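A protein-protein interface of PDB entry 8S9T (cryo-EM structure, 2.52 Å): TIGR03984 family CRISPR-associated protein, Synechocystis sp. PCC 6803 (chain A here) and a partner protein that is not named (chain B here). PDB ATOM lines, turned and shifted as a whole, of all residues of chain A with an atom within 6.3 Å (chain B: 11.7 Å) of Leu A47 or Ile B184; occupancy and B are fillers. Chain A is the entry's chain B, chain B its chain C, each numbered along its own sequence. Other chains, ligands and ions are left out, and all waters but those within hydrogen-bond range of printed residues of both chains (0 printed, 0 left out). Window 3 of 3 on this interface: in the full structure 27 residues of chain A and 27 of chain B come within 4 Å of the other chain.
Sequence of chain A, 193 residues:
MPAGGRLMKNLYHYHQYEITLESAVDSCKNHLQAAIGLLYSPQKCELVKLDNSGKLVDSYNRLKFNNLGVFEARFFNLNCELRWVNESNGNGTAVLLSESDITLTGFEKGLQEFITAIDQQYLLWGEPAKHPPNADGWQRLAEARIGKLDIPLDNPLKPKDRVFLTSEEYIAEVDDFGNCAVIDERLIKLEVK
NH1 of Arg B181 sits at hydrogen-bond distance from O of Ala B185. N of Ala B195 sits at hydrogen-bond distance from O of Ala B186.
O of Leu A123 sits at hydrogen-bond distance from N of Ala B186 (2.7 Å). The backbone NH (N) of Leu A123 sits at hydrogen-bond distance from the backbone carbonyl oxygen (O) of Ala B195. O of Pro B183 is in hydrogen-bond range of NE1 of Trp A125 (3.2 Å). The backbone carbonyl oxygen (O) of Ile B184 sits at hydrogen-bond distance from the backbone NH (N) of Trp A125. The backbone carbonyl oxygen (O) of Ala B185 lies within hydrogen-bond range of the indole nitrogen (NE1) of Trp A125, 3.2 Å away.
Leu A38 touches Ile B184 (CD1 to CD1, 3.4 Å). Tyr A40 touches Leu B182 (OH to CD1, 3.5 Å). Pro B183 touches Tyr A40. Leu A123 touches Ala B185 (O to CA, 3.2 Å). Phe B198 touches Leu A123. Leu A123 touches Pro B208. O of Ile B184 touches CA of Leu A124 (3.4 Å). Leu A124 touches Ala B186. Arg B181 touches Trp A125. N of Gly B187 touches CH2 of Trp A125, 3.9 Å away.
Of chain A, only Leu A38, Cys A45, Leu A47, Leu A124, Trp A125 and Leu A149 come within 4 Å of Ile B184. Of chain B, only Pro B183 and Ile B184 come within 4 Å of Cys A45. No residue of chain B comes within 4 Å of Glu A46. No residue of chain B comes within 4 Å of Val A48. Of chain B, only Ile B184 and Ala B186 come within 4 Å of Leu A124. Of chain B, only Arg B181, Pro B183, Ile B184, Ala B185, Ala B186 and Gly B187 come within 4 Å of Trp A125. No residue of chain B comes within 4 Å of Ile A151. No residue of chain B comes within 4 Å of Pro A152. Of the printed residues of chain A, Ala B185 touches Leu A123 and Trp A125. Printed residues of chain A within 4 Å of Leu B182: Leu A38 (3.7 Å) and Tyr A40 (3.5 Å). Of the printed residues of chain A, Phe B198 touches Leu A123. Of the printed residues of chain A, Pro B183 touches Tyr A40, Cys A45 and Trp A125. The nearest residue of chain B that does not touch Leu A47 is Pro B183 (7.3 Å).
Printed residues of chain A that touch a printed residue of chain B: Leu A38, Tyr A40, Cys A45, Leu A47, Leu A123, Leu A124, Trp A125 and Leu A149. Hydrophobic or aromatic side chains of chain A that line the printed part of chain B: Leu A38, Tyr A40, Leu A47, Leu A123, Leu A124, Trp A125 and Leu A149. Of the 15 printed residues of chain B, 10 touch a printed residue of chain A. Hydrophobic or aromatic side chains of chain B that line the printed part of chain A: Leu B182, Pro B183, Ile B184, Ala B185, Ala B186, Phe B198 and Pro B208.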
ATOM      1  N   ILE A  36      24.141  19.054  33.330  1.00  0.00           N
ATOM      2  CA  ILE A  36      23.352  20.043  32.607  1.00  0.00           C
ATOM      3  C   ILE A  36      22.606  20.895  33.619  1.00  0.00           C
ATOM      4  O   ILE A  36      21.878  20.377  34.470  1.00  0.00           O
ATOM      5  CB  ILE A  36      22.391  19.368  31.621  1.00  0.00           C
ATOM      6  CG1 ILE A  36      23.165  18.527  30.609  1.00  0.00           C
ATOM      7  CG2 ILE A  36      21.554  20.398  30.904  1.00  0.00           C
ATOM      8  CD1 ILE A  36      23.210  17.050  30.950  1.00  0.00           C
ATOM      9  N   GLY A  37      22.761  22.206  33.514  1.00  0.00           N
ATOM     10  CA  GLY A  37      21.941  23.147  34.255  1.00  0.00           C
ATOM     11  C   GLY A  37      20.829  23.728  33.402  1.00  0.00           C
ATOM     12  O   GLY A  37      20.989  23.933  32.204  1.00  0.00           O
ATOM     13  N   LEU A  38      19.693  23.962  34.036  1.00  0.00           N
ATOM     14  CA  LEU A  38      18.615  24.739  33.452  1.00  0.00           C
ATOM     15  C   LEU A  38      18.326  25.907  34.380  1.00  0.00           C
ATOM     16  O   LEU A  38      17.902  25.707  35.518  1.00  0.00           O
ATOM     17  CB  LEU A  38      17.392  23.848  33.235  1.00  0.00           C
ATOM     18  CG  LEU A  38      16.234  24.403  32.426  1.00  0.00           C
ATOM     19  CD1 LEU A  38      16.756  24.632  31.059  1.00  0.00           C
ATOM     20  CD2 LEU A  38      15.132  23.387  32.359  1.00  0.00           C
ATOM     21  N   LEU A  39      18.563  27.121  33.902  1.00  0.00           N
ATOM     22  CA  LEU A  39      18.502  28.323  34.717  1.00  0.00           C
ATOM     23  C   LEU A  39      17.271  29.122  34.322  1.00  0.00           C
ATOM     24  O   LEU A  39      16.999  29.313  33.136  1.00  0.00           O
ATOM     25  CB  LEU A  39      19.750  29.184  34.541  1.00  0.00           C
ATOM     26  CG  LEU A  39      21.115  28.528  34.681  1.00  0.00           C
ATOM     27  CD1 LEU A  39      22.195  29.573  34.510  1.00  0.00           C
ATOM     28  CD2 LEU A  39      21.249  27.826  36.004  1.00  0.00           C
ATOM     29  N   TYR A  40      16.544  29.600  35.322  1.00  0.00           N
ATOM     30  CA  TYR A  40      15.317  30.352  35.122  1.00  0.00           C
ATOM     31  C   TYR A  40      15.471  31.816  35.502  1.00  0.00           C
ATOM     32  O   TYR A  40      15.738  32.135  36.656  1.00  0.00           O
ATOM     33  CB  TYR A  40      14.184  29.735  35.936  1.00  0.00           C
ATOM     34  CG  TYR A  40      13.800  28.330  35.544  1.00  0.00           C
ATOM     35  CD1 TYR A  40      14.156  27.796  34.313  1.00  0.00           C
ATOM     36  CD2 TYR A  40      13.071  27.539  36.405  1.00  0.00           C
ATOM     37  CE1 TYR A  40      13.809  26.514  33.969  1.00  0.00           C
ATOM     38  CE2 TYR A  40      12.718  26.263  36.069  1.00  0.00           C
ATOM     39  CZ  TYR A  40      13.085  25.755  34.855  1.00  0.00           C
ATOM     40  OH  TYR A  40      12.715  24.478  34.537  1.00  0.00           O
ATOM     41  N   CYS A  45      15.454  31.237  29.610  1.00  0.00           N
ATOM     42  CA  CYS A  45      15.544  29.891  30.148  1.00  0.00           C
ATOM     43  C   CYS A  45      16.707  29.378  29.318  1.00  0.00           C
ATOM     44  O   CYS A  45      16.583  29.218  28.102  1.00  0.00           O
ATOM     45  CB  CYS A  45      14.275  29.073  29.932  1.00  0.00           C
ATOM     46  SG  CYS A  45      14.390  27.383  30.522  1.00  0.00           S
ATOM     47  N   GLU A  46      17.832  29.144  29.959  1.00  0.00           N
ATOM     48  CA  GLU A  46      19.013  28.680  29.257  1.00  0.00           C
ATOM     49  C   GLU A  46      19.583  27.403  29.844  1.00  0.00           C
ATOM     50  O   GLU A  46      19.628  27.229  31.062  1.00  0.00           O
ATOM     51  CB  GLU A  46      20.055  29.789  29.226  1.00  0.00           C
ATOM     52  CG  GLU A  46      20.557  30.220  30.552  1.00  0.00           C
ATOM     53  CD  GLU A  46      21.474  31.403  30.423  1.00  0.00           C
ATOM     54  OE1 GLU A  46      21.262  32.397  31.148  1.00  0.00           O
ATOM     55  OE2 GLU A  46      22.396  31.346  29.584  1.00  0.00           O
ATOM     56  N   LEU A  47      19.965  26.495  28.957  1.00  0.00           N
ATOM     57  CA  LEU A  47      20.753  25.354  29.359  1.00  0.00           C
ATOM     58  C   LEU A  47      22.207  25.767  29.507  1.00  0.00           C
ATOM     59  O   LEU A  47      22.705  26.635  28.793  1.00  0.00           O
ATOM     60  CB  LEU A  47      20.635  24.214  28.354  1.00  0.00           C
ATOM     61  CG  LEU A  47      19.280  23.518  28.288  1.00  0.00           C
ATOM     62  CD1 LEU A  47      18.444  24.203  27.247  1.00  0.00           C
ATOM     63  CD2 LEU A  47      19.391  22.044  28.008  1.00  0.00           C
ATOM     64  N   VAL A  48      22.884  25.132  30.460  1.00  0.00           N
ATOM     65  CA  VAL A  48      24.315  25.287  30.652  1.00  0.00           C
ATOM     66  C   VAL A  48      24.870  23.902  30.933  1.00  0.00           C
ATOM     67  O   VAL A  48      24.142  22.982  31.303  1.00  0.00           O
ATOM     68  CB  VAL A  48      24.673  26.257  31.804  1.00  0.00           C
ATOM     69  CG1 VAL A  48      24.062  27.612  31.570  1.00  0.00           C
ATOM     70  CG2 VAL A  48      24.239  25.701  33.144  1.00  0.00           C
ATOM     71  N   LYS A  49      26.173  23.754  30.758  1.00  0.00           N
ATOM     72  CA  LYS A  49      26.863  22.576  31.247  1.00  0.00           C
ATOM     73  C   LYS A  49      27.980  22.996  32.182  1.00  0.00           C
ATOM     74  O   LYS A  49      28.759  23.895  31.859  1.00  0.00           O
ATOM     75  CB  LYS A  49      27.406  21.736  30.098  1.00  0.00           C
ATOM     76  CG  LYS A  49      27.618  20.294  30.489  1.00  0.00           C
ATOM     77  CD  LYS A  49      28.302  19.514  29.409  1.00  0.00           C
ATOM     78  CE  LYS A  49      28.680  18.150  29.921  1.00  0.00           C
ATOM     79  NZ  LYS A  49      27.482  17.315  30.179  1.00  0.00           N
ATOM     80  N   ARG A  62      26.967  34.513  35.545  1.00  0.00           N
ATOM     81  CA  ARG A  62      25.891  33.682  35.026  1.00  0.00           C
ATOM     82  C   ARG A  62      24.823  33.414  36.082  1.00  0.00           C
ATOM     83  O   ARG A  62      23.629  33.379  35.769  1.00  0.00           O
ATOM     84  CB  ARG A  62      26.474  32.369  34.509  1.00  0.00           C
ATOM     85  CG  ARG A  62      25.644  31.699  33.446  1.00  0.00           C
ATOM     86  CD  ARG A  62      25.781  32.414  32.120  1.00  0.00           C
ATOM     87  NE  ARG A  62      27.098  32.186  31.548  1.00  0.00           N
ATOM     88  CZ  ARG A  62      27.423  31.109  30.843  1.00  0.00           C
ATOM     89  NH1 ARG A  62      28.652  30.971  30.366  1.00  0.00           N
ATOM     90  NH2 ARG A  62      26.516  30.172  30.606  1.00  0.00           N
ATOM     91  N   PHE A  76      21.436  18.667  36.857  1.00  0.00           N
ATOM     92  CA  PHE A  76      21.254  17.229  36.937  1.00  0.00           C
ATOM     93  C   PHE A  76      22.362  16.518  36.187  1.00  0.00           C
ATOM     94  O   PHE A  76      22.772  16.943  35.106  1.00  0.00           O
ATOM     95  CB  PHE A  76      19.870  16.776  36.419  1.00  0.00           C
ATOM     96  CG  PHE A  76      19.435  17.430  35.149  1.00  0.00           C
ATOM     97  CD1 PHE A  76      18.829  18.667  35.172  1.00  0.00           C
ATOM     98  CD2 PHE A  76      19.598  16.793  33.939  1.00  0.00           C
ATOM     99  CE1 PHE A  76      18.419  19.270  34.010  1.00  0.00           C
ATOM    100  CE2 PHE A  76      19.188  17.385  32.773  1.00  0.00           C
ATOM    101  CZ  PHE A  76      18.597  18.624  32.804  1.00  0.00           C
ATOM    102  N   LEU A 123      10.514  14.202  25.372  1.00  0.00           N
ATOM    103  CA  LEU A 123      11.012  14.633  24.076  1.00  0.00           C
ATOM    104  C   LEU A 123      11.367  16.111  24.136  1.00  0.00           C
ATOM    105  O   LEU A 123      10.536  16.931  24.526  1.00  0.00           O
ATOM    106  CB  LEU A 123       9.957  14.368  23.013  1.00  0.00           C
ATOM    107  CG  LEU A 123      10.218  14.830  21.590  1.00  0.00           C
ATOM    108  CD1 LEU A 123      11.388  14.090  20.974  1.00  0.00           C
ATOM    109  CD2 LEU A 123       8.971  14.632  20.799  1.00  0.00           C
ATOM    110  N   LEU A 124      12.598  16.451  23.778  1.00  0.00           N
ATOM    111  CA  LEU A 124      13.007  17.842  23.647  1.00  0.00           C
ATOM    112  C   LEU A 124      12.417  18.509  22.400  1.00  0.00           C
ATOM    113  O   LEU A 124      12.088  17.857  21.415  1.00  0.00           O
ATOM    114  CB  LEU A 124      14.525  17.966  23.626  1.00  0.00           C
ATOM    115  CG  LEU A 124      15.269  17.616  24.915  1.00  0.00           C
ATOM    116  CD1 LEU A 124      16.647  18.247  24.933  1.00  0.00           C
ATOM    117  CD2 LEU A 124      14.498  17.854  26.196  1.00  0.00           C
ATOM    118  N   TRP A 125      12.293  19.830  22.461  1.00  0.00           N
ATOM    119  CA  TRP A 125      11.847  20.638  21.328  1.00  0.00           C
ATOM    120  C   TRP A 125      12.822  20.583  20.157  1.00  0.00           C
ATOM    121  O   TRP A 125      14.006  20.886  20.315  1.00  0.00           O
ATOM    122  CB  TRP A 125      11.736  22.110  21.729  1.00  0.00           C
ATOM    123  CG  TRP A 125      10.604  22.577  22.521  1.00  0.00           C
ATOM    124  CD1 TRP A 125      10.659  23.118  23.752  1.00  0.00           C
ATOM    125  CD2 TRP A 125       9.242  22.629  22.116  1.00  0.00           C
ATOM    126  NE1 TRP A 125       9.413  23.476  24.166  1.00  0.00           N
ATOM    127  CE2 TRP A 125       8.518  23.183  23.176  1.00  0.00           C
ATOM    128  CE3 TRP A 125       8.557  22.229  20.973  1.00  0.00           C
ATOM    129  CZ2 TRP A 125       7.149  23.353  23.129  1.00  0.00           C
ATOM    130  CZ3 TRP A 125       7.210  22.395  20.929  1.00  0.00           C
ATOM    131  CH2 TRP A 125       6.515  22.953  21.996  1.00  0.00           C
ATOM    132  N   GLY A 126      12.332  20.204  18.984  1.00  0.00           N
ATOM    133  CA  GLY A 126      13.098  20.372  17.769  1.00  0.00           C
ATOM    134  C   GLY A 126      13.764  19.109  17.249  1.00  0.00           C
ATOM    135  O   GLY A 126      13.961  18.124  17.960  1.00  0.00           O
ATOM    136  N   TRP A 138      28.075  21.164  22.169  1.00  0.00           N
ATOM    137  CA  TRP A 138      26.762  21.752  21.976  1.00  0.00           C
ATOM    138  C   TRP A 138      26.204  21.310  20.638  1.00  0.00           C
ATOM    139  O   TRP A 138      26.934  21.162  19.658  1.00  0.00           O
ATOM    140  CB  TRP A 138      26.820  23.277  22.051  1.00  0.00           C
ATOM    141  CG  TRP A 138      27.027  23.758  23.440  1.00  0.00           C
ATOM    142  CD1 TRP A 138      28.211  23.894  24.084  1.00  0.00           C
ATOM    143  CD2 TRP A 138      26.018  24.191  24.358  1.00  0.00           C
ATOM    144  NE1 TRP A 138      28.009  24.360  25.357  1.00  0.00           N
ATOM    145  CE2 TRP A 138      26.669  24.555  25.549  1.00  0.00           C
ATOM    146  CE3 TRP A 138      24.629  24.300  24.292  1.00  0.00           C
ATOM    147  CZ2 TRP A 138      25.980  25.021  26.660  1.00  0.00           C
ATOM    148  CZ3 TRP A 138      23.951  24.758  25.393  1.00  0.00           C
ATOM    149  CH2 TRP A 138      24.623  25.113  26.563  1.00  0.00           C
ATOM    150  N   LEU A 149      17.142  25.528  19.508  1.00  0.00           N
ATOM    151  CA  LEU A 149      17.406  25.161  20.893  1.00  0.00           C
ATOM    152  C   LEU A 149      18.795  24.541  20.951  1.00  0.00           C
ATOM    153  O   LEU A 149      18.986  23.413  20.495  1.00  0.00           O
ATOM    154  CB  LEU A 149      16.351  24.192  21.421  1.00  0.00           C
ATOM    155  CG  LEU A 149      16.570  23.627  22.825  1.00  0.00           C
ATOM    156  CD1 LEU A 149      16.426  24.688  23.889  1.00  0.00           C
ATOM    157  CD2 LEU A 149      15.642  22.462  23.087  1.00  0.00           C
ATOM    158  N   ASP A 150      19.766  25.268  21.488  1.00  0.00           N
ATOM    159  CA  ASP A 150      21.082  24.690  21.721  1.00  0.00           C
ATOM    160  C   ASP A 150      21.084  23.875  23.006  1.00  0.00           C
ATOM    161  O   ASP A 150      20.683  24.361  24.066  1.00  0.00           O
ATOM    162  CB  ASP A 150      22.160  25.768  21.792  1.00  0.00           C
ATOM    163  CG  ASP A 150      22.326  26.511  20.494  1.00  0.00           C
ATOM    164  OD1 ASP A 150      21.545  26.266  19.556  1.00  0.00           O
ATOM    165  OD2 ASP A 150      23.250  27.345  20.411  1.00  0.00           O
ATOM    166  N   ILE A 151      21.568  22.642  22.910  1.00  0.00           N
ATOM    167  CA  ILE A 151      21.541  21.701  24.018  1.00  0.00           C
ATOM    168  C   ILE A 151      22.968  21.236  24.255  1.00  0.00           C
ATOM    169  O   ILE A 151      23.719  21.043  23.292  1.00  0.00           O
ATOM    170  CB  ILE A 151      20.611  20.515  23.730  1.00  0.00           C
ATOM    171  CG1 ILE A 151      21.094  19.748  22.504  1.00  0.00           C
ATOM    172  CG2 ILE A 151      19.201  20.999  23.487  1.00  0.00           C
ATOM    173  CD1 ILE A 151      20.491  18.402  22.352  1.00  0.00           C
ATOM    174  N   PRO A 152      23.387  21.044  25.502  1.00  0.00           N
ATOM    175  CA  PRO A 152      24.758  20.584  25.773  1.00  0.00           C
ATOM    176  C   PRO A 152      24.902  19.081  25.562  1.00  0.00           C
ATOM    177  O   PRO A 152      24.862  18.266  26.476  1.00  0.00           O
ATOM    178  CB  PRO A 152      24.965  20.998  27.228  1.00  0.00           C
ATOM    179  CG  PRO A 152      23.612  20.937  27.811  1.00  0.00           C
ATOM    180  CD  PRO A 152      22.643  21.306  26.745  1.00  0.00           C
ATOM    181  N   LEU A 165      15.051  14.044  27.197  1.00  0.00           N
ATOM    182  CA  LEU A 165      15.470  14.140  28.587  1.00  0.00           C
ATOM    183  C   LEU A 165      14.908  12.948  29.355  1.00  0.00           C
ATOM    184  O   LEU A 165      13.692  12.786  29.458  1.00  0.00           O
ATOM    185  CB  LEU A 165      15.000  15.464  29.183  1.00  0.00           C
ATOM    186  CG  LEU A 165      15.645  16.075  30.426  1.00  0.00           C
ATOM    187  CD1 LEU A 165      15.088  17.465  30.616  1.00  0.00           C
ATOM    188  CD2 LEU A 165      15.389  15.266  31.659  1.00  0.00           C
ATOM    189  N   LEU A 190      20.393  14.018  28.968  1.00  0.00           N
ATOM    190  CA  LEU A 190      19.966  14.035  27.578  1.00  0.00           C
ATOM    191  C   LEU A 190      20.446  12.791  26.852  1.00  0.00           C
ATOM    192  O   LEU A 190      21.601  12.386  26.977  1.00  0.00           O
ATOM    193  CB  LEU A 190      20.482  15.283  26.868  1.00  0.00           C
ATOM    194  CG  LEU A 190      20.091  16.634  27.461  1.00  0.00           C
ATOM    195  CD1 LEU A 190      20.525  17.743  26.550  1.00  0.00           C
ATOM    196  CD2 LEU A 190      18.602  16.700  27.687  1.00  0.00           C
ATOM    197  N   LEU B 180       5.540  16.417  34.572  1.00  0.00           N
ATOM    198  CA  LEU B 180       5.520  17.872  34.544  1.00  0.00           C
ATOM    199  C   LEU B 180       6.361  18.451  33.420  1.00  0.00           C
ATOM    200  O   LEU B 180       7.481  18.005  33.160  1.00  0.00           O
ATOM    201  CB  LEU B 180       5.996  18.459  35.871  1.00  0.00           C
ATOM    202  CG  LEU B 180       5.165  18.192  37.120  1.00  0.00           C
ATOM    203  CD1 LEU B 180       5.872  18.697  38.346  1.00  0.00           C
ATOM    204  CD2 LEU B 180       3.844  18.891  36.975  1.00  0.00           C
ATOM    205  N   ARG B 181       5.795  19.469  32.775  1.00  0.00           N
ATOM    206  CA  ARG B 181       6.473  20.224  31.733  1.00  0.00           C
ATOM    207  C   ARG B 181       7.731  20.939  32.192  1.00  0.00           C
ATOM    208  O   ARG B 181       7.746  21.645  33.202  1.00  0.00           O
ATOM    209  CB  ARG B 181       5.554  21.223  31.038  1.00  0.00           C
ATOM    210  CG  ARG B 181       6.178  21.635  29.698  1.00  0.00           C
ATOM    211  CD  ARG B 181       5.965  20.693  28.530  1.00  0.00           C
ATOM    212  NE  ARG B 181       4.794  21.011  27.736  1.00  0.00           N
ATOM    213  CZ  ARG B 181       4.847  21.668  26.587  1.00  0.00           C
ATOM    214  NH1 ARG B 181       6.011  22.035  26.093  1.00  0.00           N
ATOM    215  NH2 ARG B 181       3.741  21.942  25.918  1.00  0.00           N
ATOM    216  N   LEU B 182       8.782  20.754  31.406  1.00  0.00           N
ATOM    217  CA  LEU B 182      10.075  21.335  31.576  1.00  0.00           C
ATOM    218  C   LEU B 182      10.170  22.232  30.356  1.00  0.00           C
ATOM    219  O   LEU B 182       9.778  21.803  29.265  1.00  0.00           O
ATOM    220  CB  LEU B 182      11.178  20.275  31.544  1.00  0.00           C
ATOM    221  CG  LEU B 182      11.972  19.918  32.795  1.00  0.00           C
ATOM    222  CD1 LEU B 182      12.416  21.152  33.531  1.00  0.00           C
ATOM    223  CD2 LEU B 182      11.157  19.033  33.693  1.00  0.00           C
ATOM    224  N   PRO B 183      10.596  23.484  30.499  1.00  0.00           N
ATOM    225  CA  PRO B 183      10.601  24.400  29.343  1.00  0.00           C
ATOM    226  C   PRO B 183      11.177  23.851  28.047  1.00  0.00           C
ATOM    227  O   PRO B 183      10.783  24.303  26.972  1.00  0.00           O
ATOM    228  CB  PRO B 183      11.429  25.568  29.871  1.00  0.00           C
ATOM    229  CG  PRO B 183      11.142  25.570  31.310  1.00  0.00           C
ATOM    230  CD  PRO B 183      11.009  24.159  31.735  1.00  0.00           C
ATOM    231  N   ILE B 184      12.082  22.878  28.108  1.00  0.00           N
ATOM    232  CA  ILE B 184      12.723  22.354  26.909  1.00  0.00           C
ATOM    233  C   ILE B 184      12.053  21.094  26.374  1.00  0.00           C
ATOM    234  O   ILE B 184      12.300  20.716  25.220  1.00  0.00           O
ATOM    235  CB  ILE B 184      14.232  22.185  27.194  1.00  0.00           C
ATOM    236  CG1 ILE B 184      14.904  23.534  27.028  1.00  0.00           C
ATOM    237  CG2 ILE B 184      14.920  21.217  26.283  1.00  0.00           C
ATOM    238  CD1 ILE B 184      14.930  24.341  28.239  1.00  0.00           C
ATOM    239  N   ALA B 185      11.134  20.500  27.121  1.00  0.00           N
ATOM    240  CA  ALA B 185      10.325  19.413  26.594  1.00  0.00           C
ATOM    241  C   ALA B 185       9.263  19.909  25.621  1.00  0.00           C
ATOM    242  O   ALA B 185       8.613  20.925  25.849  1.00  0.00           O
ATOM    243  CB  ALA B 185       9.663  18.641  27.732  1.00  0.00           C
ATOM    244  N   ALA B 186       9.096  19.172  24.533  1.00  0.00           N
ATOM    245  CA  ALA B 186       8.085  19.448  23.535  1.00  0.00           C
ATOM    246  C   ALA B 186       6.732  19.011  24.080  1.00  0.00           C
ATOM    247  O   ALA B 186       6.644  18.257  25.051  1.00  0.00           O
ATOM    248  CB  ALA B 186       8.407  18.725  22.236  1.00  0.00           C
ATOM    249  N   GLY B 187       5.663  19.445  23.442  1.00  0.00           N
ATOM    250  CA  GLY B 187       4.402  18.987  23.964  1.00  0.00           C
ATOM    251  C   GLY B 187       3.686  17.909  23.187  1.00  0.00           C
ATOM    252  O   GLY B 187       3.958  17.667  22.014  1.00  0.00           O
ATOM    253  N   CYS B 188       2.783  17.227  23.876  1.00  0.00           N
ATOM    254  CA  CYS B 188       1.935  16.229  23.255  1.00  0.00           C
ATOM    255  C   CYS B 188       1.113  16.859  22.144  1.00  0.00           C
ATOM    256  O   CYS B 188       0.722  18.022  22.219  1.00  0.00           O
ATOM    257  CB  CYS B 188       1.030  15.587  24.298  1.00  0.00           C
ATOM    258  SG  CYS B 188      -0.023  14.285  23.692  1.00  0.00           S
ATOM    259  N   LEU B 193       0.103  17.629  28.343  1.00  0.00           N
ATOM    260  CA  LEU B 193       1.317  17.099  28.938  1.00  0.00           C
ATOM    261  C   LEU B 193       2.509  17.262  28.009  1.00  0.00           C
ATOM    262  O   LEU B 193       2.348  17.471  26.805  1.00  0.00           O
ATOM    263  CB  LEU B 193       1.120  15.631  29.288  1.00  0.00           C
ATOM    264  CG  LEU B 193       0.066  15.297  30.338  1.00  0.00           C
ATOM    265  CD1 LEU B 193       0.106  13.829  30.591  1.00  0.00           C
ATOM    266  CD2 LEU B 193       0.286  16.038  31.613  1.00  0.00           C
ATOM    267  N   PRO B 194       3.729  17.208  28.543  1.00  0.00           N
ATOM    268  CA  PRO B 194       4.898  17.095  27.671  1.00  0.00           C
ATOM    269  C   PRO B 194       4.871  15.816  26.846  1.00  0.00           C
ATOM    270  O   PRO B 194       4.413  14.764  27.294  1.00  0.00           O
ATOM    271  CB  PRO B 194       6.066  17.103  28.657  1.00  0.00           C
ATOM    272  CG  PRO B 194       5.504  16.578  29.894  1.00  0.00           C
ATOM    273  CD  PRO B 194       4.110  17.104  29.959  1.00  0.00           C
ATOM    274  N   ALA B 195       5.409  15.910  25.637  1.00  0.00           N
ATOM    275  CA  ALA B 195       5.587  14.736  24.805  1.00  0.00           C
ATOM    276  C   ALA B 195       6.674  13.847  25.377  1.00  0.00           C
ATOM    277  O   ALA B 195       7.617  14.309  26.019  1.00  0.00           O
ATOM    278  CB  ALA B 195       5.922  15.138  23.373  1.00  0.00           C
ATOM    279  N   SER B 196       6.511  12.549  25.165  1.00  0.00           N
ATOM    280  CA  SER B 196       7.386  11.567  25.778  1.00  0.00           C
ATOM    281  C   SER B 196       7.889  10.595  24.727  1.00  0.00           C
ATOM    282  O   SER B 196       9.009  10.091  24.825  1.00  0.00           O
ATOM    283  CB  SER B 196       6.655  10.850  26.900  1.00  0.00           C
ATOM    284  OG  SER B 196       7.393   9.746  27.376  1.00  0.00           O
ATOM    285  N   PHE B 198       6.493   8.978  20.437  1.00  0.00           N
ATOM    286  CA  PHE B 198       5.820   9.242  19.178  1.00  0.00           C
ATOM    287  C   PHE B 198       4.725   8.224  18.918  1.00  0.00           C
ATOM    288  O   PHE B 198       4.822   7.064  19.313  1.00  0.00           O
ATOM    289  CB  PHE B 198       6.805   9.243  18.014  1.00  0.00           C
ATOM    290  CG  PHE B 198       7.715  10.418  18.015  1.00  0.00           C
ATOM    291  CD1 PHE B 198       7.333  11.593  17.410  1.00  0.00           C
ATOM    292  CD2 PHE B 198       8.946  10.352  18.622  1.00  0.00           C
ATOM    293  CE1 PHE B 198       8.156  12.673  17.424  1.00  0.00           C
ATOM    294  CE2 PHE B 198       9.772  11.424  18.626  1.00  0.00           C
ATOM    295  CZ  PHE B 198       9.380  12.585  18.031  1.00  0.00           C
ATOM    296  N   PRO B 208       4.360  13.622  18.118  1.00  0.00           N
ATOM    297  CA  PRO B 208       4.763  13.444  19.516  1.00  0.00           C
ATOM    298  C   PRO B 208       3.565  13.334  20.451  1.00  0.00           C
ATOM    299  O   PRO B 208       2.605  14.098  20.357  1.00  0.00           O
ATOM    300  CB  PRO B 208       5.584  14.702  19.792  1.00  0.00           C
ATOM    301  CG  PRO B 208       5.003  15.704  18.896  1.00  0.00           C
ATOM    302  CD  PRO B 208       4.614  14.991  17.648  1.00  0.00           C
